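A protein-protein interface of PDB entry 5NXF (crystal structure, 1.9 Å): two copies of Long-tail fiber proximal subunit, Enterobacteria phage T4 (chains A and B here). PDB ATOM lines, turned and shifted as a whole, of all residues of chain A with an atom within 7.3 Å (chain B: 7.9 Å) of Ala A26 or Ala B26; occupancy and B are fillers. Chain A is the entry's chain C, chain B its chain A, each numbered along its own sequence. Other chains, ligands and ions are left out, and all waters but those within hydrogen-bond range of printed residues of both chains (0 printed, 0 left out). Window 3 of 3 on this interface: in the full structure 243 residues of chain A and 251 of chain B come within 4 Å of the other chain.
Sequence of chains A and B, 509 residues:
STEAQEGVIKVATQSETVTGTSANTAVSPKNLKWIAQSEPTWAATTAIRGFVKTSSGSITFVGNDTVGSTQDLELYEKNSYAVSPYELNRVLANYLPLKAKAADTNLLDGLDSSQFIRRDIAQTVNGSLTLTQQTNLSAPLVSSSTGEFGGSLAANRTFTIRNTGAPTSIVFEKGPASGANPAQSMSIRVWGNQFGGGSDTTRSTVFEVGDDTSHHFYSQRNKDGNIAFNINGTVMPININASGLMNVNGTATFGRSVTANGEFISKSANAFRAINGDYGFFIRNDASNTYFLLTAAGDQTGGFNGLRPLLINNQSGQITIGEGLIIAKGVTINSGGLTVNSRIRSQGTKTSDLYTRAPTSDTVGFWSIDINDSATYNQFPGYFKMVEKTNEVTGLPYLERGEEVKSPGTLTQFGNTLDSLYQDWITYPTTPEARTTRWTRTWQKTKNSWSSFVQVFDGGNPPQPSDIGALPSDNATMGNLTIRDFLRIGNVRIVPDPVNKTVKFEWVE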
ATOM      1  N   SER A  15      -1.770 -28.777 -32.929  1.00  0.00           N
ATOM      2  CA  SER A  15      -0.311 -28.793 -33.252  1.00  0.00           C
ATOM      3  C   SER A  15       0.496 -28.134 -32.126  1.00  0.00           C
ATOM      4  O   SER A  15      -0.088 -27.637 -31.163  1.00  0.00           O
ATOM      5  CB  SER A  15      -0.075 -28.074 -34.585  1.00  0.00           C
ATOM      6  OG  SER A  15       1.306 -27.866 -34.845  1.00  0.00           O
ATOM      7  N   VAL A  18       0.809 -23.976 -31.355  1.00  0.00           N
ATOM      8  CA  VAL A  18       0.140 -23.248 -30.261  1.00  0.00           C
ATOM      9  C   VAL A  18       1.052 -22.100 -29.765  1.00  0.00           C
ATOM     10  O   VAL A  18       0.564 -21.092 -29.243  1.00  0.00           O
ATOM     11  CB  VAL A  18      -0.279 -24.188 -29.082  1.00  0.00           C
ATOM     12  CG1 VAL A  18      -1.066 -23.436 -28.014  1.00  0.00           C
ATOM     13  CG2 VAL A  18      -1.131 -25.359 -29.563  1.00  0.00           C
ATOM     14  N   SER A  22      -3.142 -19.212 -33.204  1.00  0.00           N
ATOM     15  CA  SER A  22      -4.311 -18.760 -33.962  1.00  0.00           C
ATOM     16  C   SER A  22      -5.553 -19.528 -33.502  1.00  0.00           C
ATOM     17  O   SER A  22      -5.462 -20.425 -32.669  1.00  0.00           O
ATOM     18  CB  SER A  22      -4.093 -18.985 -35.460  1.00  0.00           C
ATOM     19  OG  SER A  22      -2.923 -18.331 -35.916  1.00  0.00           O
ATOM     20  N   ALA A  23      -6.715 -19.168 -34.041  1.00  0.00           N
ATOM     21  CA  ALA A  23      -7.933 -19.974 -33.867  1.00  0.00           C
ATOM     22  C   ALA A  23      -7.820 -21.211 -34.778  1.00  0.00           C
ATOM     23  O   ALA A  23      -6.707 -21.593 -35.161  1.00  0.00           O
ATOM     24  CB  ALA A  23      -9.174 -19.148 -34.194  1.00  0.00           C
ATOM     25  N   ASN A  24      -8.948 -21.859 -35.091  1.00  0.00           N
ATOM     26  CA  ASN A  24      -9.003 -22.932 -36.113  1.00  0.00           C
ATOM     27  C   ASN A  24      -8.349 -24.275 -35.694  1.00  0.00           C
ATOM     28  O   ASN A  24      -8.232 -25.186 -36.520  1.00  0.00           O
ATOM     29  CB  ASN A  24      -8.389 -22.424 -37.445  1.00  0.00           C
ATOM     30  CG  ASN A  24      -8.974 -23.094 -38.684  1.00  0.00           C
ATOM     31  OD1 ASN A  24      -9.888 -23.915 -38.607  1.00  0.00           O
ATOM     32  ND2 ASN A  24      -8.437 -22.732 -39.845  1.00  0.00           N
ATOM     33  N   THR A  25      -7.943 -24.398 -34.424  1.00  0.00           N
ATOM     34  CA  THR A  25      -7.322 -25.623 -33.886  1.00  0.00           C
ATOM     35  C   THR A  25      -7.627 -25.753 -32.388  1.00  0.00           C
ATOM     36  O   THR A  25      -7.968 -24.765 -31.732  1.00  0.00           O
ATOM     37  CB  THR A  25      -5.781 -25.647 -34.093  1.00  0.00           C
ATOM     38  OG1 THR A  25      -5.238 -24.335 -33.898  1.00  0.00           O
ATOM     39  CG2 THR A  25      -5.409 -26.146 -35.490  1.00  0.00           C
ATOM     40  N   ALA A  26      -7.516 -26.982 -31.872  1.00  0.00           N
ATOM     41  CA  ALA A  26      -7.594 -27.266 -30.431  1.00  0.00           C
ATOM     42  C   ALA A  26      -6.201 -27.609 -29.898  1.00  0.00           C
ATOM     43  O   ALA A  26      -5.325 -28.054 -30.657  1.00  0.00           O
ATOM     44  CB  ALA A  26      -8.559 -28.409 -30.160  1.00  0.00           C
ATOM     45  N   VAL A  27      -6.010 -27.388 -28.595  1.00  0.00           N
ATOM     46  CA  VAL A  27      -4.731 -27.654 -27.915  1.00  0.00           C
ATOM     47  C   VAL A  27      -4.837 -28.960 -27.123  1.00  0.00           C
ATOM     48  O   VAL A  27      -5.855 -29.230 -26.471  1.00  0.00           O
ATOM     49  CB  VAL A  27      -4.315 -26.495 -26.968  1.00  0.00           C
ATOM     50  CG1 VAL A  27      -2.854 -26.639 -26.547  1.00  0.00           C
ATOM     51  CG2 VAL A  27      -4.550 -25.142 -27.634  1.00  0.00           C
ATOM     52  N   SER A  28      -3.774 -29.759 -27.190  1.00  0.00           N
ATOM     53  CA  SER A  28      -3.698 -31.051 -26.506  1.00  0.00           C
ATOM     54  C   SER A  28      -3.063 -30.893 -25.124  1.00  0.00           C
ATOM     55  O   SER A  28      -2.335 -29.915 -24.897  1.00  0.00           O
ATOM     56  CB  SER A  28      -2.861 -32.016 -27.341  1.00  0.00           C
ATOM     57  OG  SER A  28      -1.558 -31.497 -27.568  1.00  0.00           O
ATOM     58  N   PRO A  29      -3.333 -31.846 -24.196  1.00  0.00           N
ATOM     59  CA  PRO A  29      -2.576 -31.909 -22.932  1.00  0.00           C
ATOM     60  C   PRO A  29      -1.054 -31.926 -23.124  1.00  0.00           C
ATOM     61  O   PRO A  29      -0.331 -31.378 -22.291  1.00  0.00           O
ATOM     62  CB  PRO A  29      -3.062 -33.215 -22.294  1.00  0.00           C
ATOM     63  CG  PRO A  29      -4.463 -33.358 -22.790  1.00  0.00           C
ATOM     64  CD  PRO A  29      -4.455 -32.807 -24.196  1.00  0.00           C
ATOM     65  N   ASN A  31       0.631 -30.322 -25.695  1.00  0.00           N
ATOM     66  CA  ASN A  31       1.028 -28.939 -26.027  1.00  0.00           C
ATOM     67  C   ASN A  31       0.790 -27.894 -24.919  1.00  0.00           C
ATOM     68  O   ASN A  31       1.480 -26.871 -24.900  1.00  0.00           O
ATOM     69  CB  ASN A  31       0.364 -28.487 -27.327  1.00  0.00           C
ATOM     70  CG  ASN A  31       0.879 -29.245 -28.526  1.00  0.00           C
ATOM     71  OD1 ASN A  31       2.080 -29.505 -28.646  1.00  0.00           O
ATOM     72  ND2 ASN A  31      -0.026 -29.614 -29.420  1.00  0.00           N
ATOM     73  N   SER B  15     -11.741 -35.301 -19.053  1.00  0.00           N
ATOM     74  CA  SER B  15     -11.366 -35.697 -17.664  1.00  0.00           C
ATOM     75  C   SER B  15      -9.935 -35.264 -17.344  1.00  0.00           C
ATOM     76  O   SER B  15      -9.214 -34.765 -18.212  1.00  0.00           O
ATOM     77  CB  SER B  15     -11.516 -37.218 -17.490  1.00  0.00           C
ATOM     78  OG  SER B  15     -12.875 -37.573 -17.303  1.00  0.00           O
ATOM     79  N   VAL B  18      -5.883 -34.671 -18.542  1.00  0.00           N
ATOM     80  CA  VAL B  18      -5.159 -33.426 -18.864  1.00  0.00           C
ATOM     81  C   VAL B  18      -4.046 -33.148 -17.845  1.00  0.00           C
ATOM     82  O   VAL B  18      -2.988 -32.615 -18.206  1.00  0.00           O
ATOM     83  CB  VAL B  18      -6.114 -32.196 -18.952  1.00  0.00           C
ATOM     84  CG1 VAL B  18      -5.351 -30.951 -19.401  1.00  0.00           C
ATOM     85  CG2 VAL B  18      -7.295 -32.470 -19.888  1.00  0.00           C
ATOM     86  N   ALA B  23      -0.960 -36.581 -24.127  1.00  0.00           N
ATOM     87  CA  ALA B  23      -2.205 -37.066 -24.771  1.00  0.00           C
ATOM     88  C   ALA B  23      -2.477 -36.150 -25.962  1.00  0.00           C
ATOM     89  O   ALA B  23      -1.956 -35.029 -26.011  1.00  0.00           O
ATOM     90  CB  ALA B  23      -3.411 -37.070 -23.831  1.00  0.00           C
ATOM     91  N   ASN B  24      -3.269 -36.637 -26.920  1.00  0.00           N
ATOM     92  CA  ASN B  24      -3.738 -35.824 -28.058  1.00  0.00           C
ATOM     93  C   ASN B  24      -5.268 -35.883 -28.204  1.00  0.00           C
ATOM     94  O   ASN B  24      -5.813 -36.113 -29.289  1.00  0.00           O
ATOM     95  CB  ASN B  24      -3.010 -36.214 -29.352  1.00  0.00           C
ATOM     96  CG  ASN B  24      -1.587 -35.680 -29.401  1.00  0.00           C
ATOM     97  OD1 ASN B  24      -0.739 -36.058 -28.593  1.00  0.00           O
ATOM     98  ND2 ASN B  24      -1.321 -34.790 -30.350  1.00  0.00           N
ATOM     99  N   THR B  25      -5.942 -35.684 -27.069  1.00  0.00           N
ATOM    100  CA  THR B  25      -7.328 -35.228 -27.034  1.00  0.00           C
ATOM    101  C   THR B  25      -7.267 -33.683 -26.991  1.00  0.00           C
ATOM    102  O   THR B  25      -6.193 -33.112 -27.203  1.00  0.00           O
ATOM    103  CB  THR B  25      -8.070 -35.818 -25.817  1.00  0.00           C
ATOM    104  OG1 THR B  25      -7.374 -35.475 -24.612  1.00  0.00           O
ATOM    105  CG2 THR B  25      -8.152 -37.333 -25.936  1.00  0.00           C
ATOM    106  N   ALA B  26      -8.400 -33.012 -26.759  1.00  0.00           N
ATOM    107  CA  ALA B  26      -8.437 -31.543 -26.635  1.00  0.00           C
ATOM    108  C   ALA B  26      -8.644 -31.135 -25.179  1.00  0.00           C
ATOM    109  O   ALA B  26      -9.395 -31.793 -24.448  1.00  0.00           O
ATOM    110  CB  ALA B  26      -9.544 -30.956 -27.502  1.00  0.00           C
ATOM    111  N   VAL B  27      -7.973 -30.057 -24.765  1.00  0.00           N
ATOM    112  CA  VAL B  27      -8.175 -29.475 -23.424  1.00  0.00           C
ATOM    113  C   VAL B  27      -9.456 -28.616 -23.379  1.00  0.00           C
ATOM    114  O   VAL B  27      -9.757 -27.883 -24.332  1.00  0.00           O
ATOM    115  CB  VAL B  27      -6.937 -28.665 -22.935  1.00  0.00           C
ATOM    116  CG1 VAL B  27      -5.697 -29.555 -22.900  1.00  0.00           C
ATOM    117  CG2 VAL B  27      -6.684 -27.406 -23.779  1.00  0.00           C
ATOM    118  N   SER B  28     -10.206 -28.731 -22.277  1.00  0.00           N
ATOM    119  CA  SER B  28     -11.471 -28.018 -22.085  1.00  0.00           C
ATOM    120  C   SER B  28     -11.301 -26.757 -21.219  1.00  0.00           C
ATOM    121  O   SER B  28     -10.248 -26.565 -20.611  1.00  0.00           O
ATOM    122  CB  SER B  28     -12.494 -28.947 -21.424  1.00  0.00           C
ATOM    123  OG  SER B  28     -11.989 -29.519 -20.230  1.00  0.00           O
ATOM    124  N   PRO B  29     -12.338 -25.895 -21.171  1.00  0.00           N
ATOM    125  CA  PRO B  29     -12.469 -24.815 -20.183  1.00  0.00           C
ATOM    126  C   PRO B  29     -12.394 -25.259 -18.713  1.00  0.00           C
ATOM    127  O   PRO B  29     -11.685 -24.629 -17.924  1.00  0.00           O
ATOM    128  CB  PRO B  29     -13.858 -24.244 -20.480  1.00  0.00           C
ATOM    129  CG  PRO B  29     -14.036 -24.459 -21.938  1.00  0.00           C
ATOM    130  CD  PRO B  29     -13.311 -25.733 -22.271  1.00  0.00           C
ATOM    131  N   ASN B  31     -11.121 -28.119 -17.405  1.00  0.00           N
ATOM    132  CA  ASN B  31      -9.796 -28.698 -17.127  1.00  0.00           C
ATOM    133  C   ASN B  31      -8.656 -27.663 -17.123  1.00  0.00           C
ATOM    134  O   ASN B  31      -7.682 -27.839 -16.388  1.00  0.00           O
ATOM    135  CB  ASN B  31      -9.455 -29.823 -18.126  1.00  0.00           C
ATOM    136  CG  ASN B  31     -10.327 -31.060 -17.955  1.00  0.00           C
ATOM    137  OD1 ASN B  31     -10.784 -31.373 -16.853  1.00  0.00           O
ATOM    138  ND2 ASN B  31     -10.547 -31.778 -19.055  1.00  0.00           N
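O of Val A27 is in hydrogen-bond range of N of Val B27, at 2.8 Å.
ND2 of Asn A31 is in hydrogen-bond range of OG of Ser A28, at 3.1 Å.
Among the printed residues, pairs that only touch across the chains: Ala A26 with Ala B26 (3.8 Å), Val A27 with Thr B25 (3.96 Å), Val A27 with Ala B26 (3.5 Å), Ser A28 with Ala B23 (3.4 Å), Ser A28 with Asn B24 (3.97 Å), Ser A28 with Thr B25 (3.3 Å), Ser A28 with Val B27 (3.7 Å), Pro A29 with Val B18 (3.99 Å), Pro A29 with Ala B23 (3.8 Å), Pro A29 with Thr B25 (3.5 Å) and Pro A29 with Val B27 (3.5 Å).
Printed residues of chain B within 4 Å of Ala A26: Ala B26.
Of the printed residues of chain A, Ala B26 touches Ala A26 and Val A27.
Printed residues of chain B within 4 Å of Ser A28: Ala B23 (3.4 Å), Asn B24 (3.97 Å), Thr B25 (3.3 Å) and Val B27 (3.7 Å).
Of the printed residues of chain A, Val B27 touches Val A27 (2.8 Å), Ser A28 (3.7 Å) and Pro A29 (3.5 Å).
Of the printed residues of chain A, Thr B25 touches Val A27 (3.96 Å), Ser A28 (3.3 Å) and Pro A29 (3.5 Å).
Printed residues of chain B within 4 Å of Val A27: Thr B25 (3.96 Å), Ala B26 (3.5 Å) and Val B27 (2.8 Å).
Pro B29 touches none of the printed residues of chain A.
Ser A22 touches none of the printed residues of chain B.
The nearest residue of chain A that does not touch Ala B26 is Pro A29 (4.6 Å).
The nearest printed residue of chain B that does not touch Val A27 is Ser B28 (6.1 Å).
Hydrophobic or aromatic side chains of chain B within 4 Å of the printed part of chain A: Ala B23, Ala B26 and Val B27.
Of the 11 printed residues of chain A, 4 touch a printed residue of chain B.
Among the printed residues, 12 pairs touch across the chains.
Ser A28 touches Asn B24, but with the chains exchanged Asn A24 does not touch Ser B28 (14.3 Å).
Ser A28 touches Thr B25, but with the chains exchanged Thr A25 does not touch Ser B28 (10.5 Å).
Ser A28 touches Val B27, but with the chains exchanged Val A27 does not touch Ser B28 (6.1 Å).
Pro A29 touches Val B27, but with the chains exchanged Val A27 does not touch Pro B29 (9.0 Å).
Positions printed for both chains: 15, 18, 23, 24, 25, 26, 27, 28, 29 and 31.
Of the 12 pairs that touch across the chains among the printed residues, 2 have their exchanged pair printed and touching as well.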
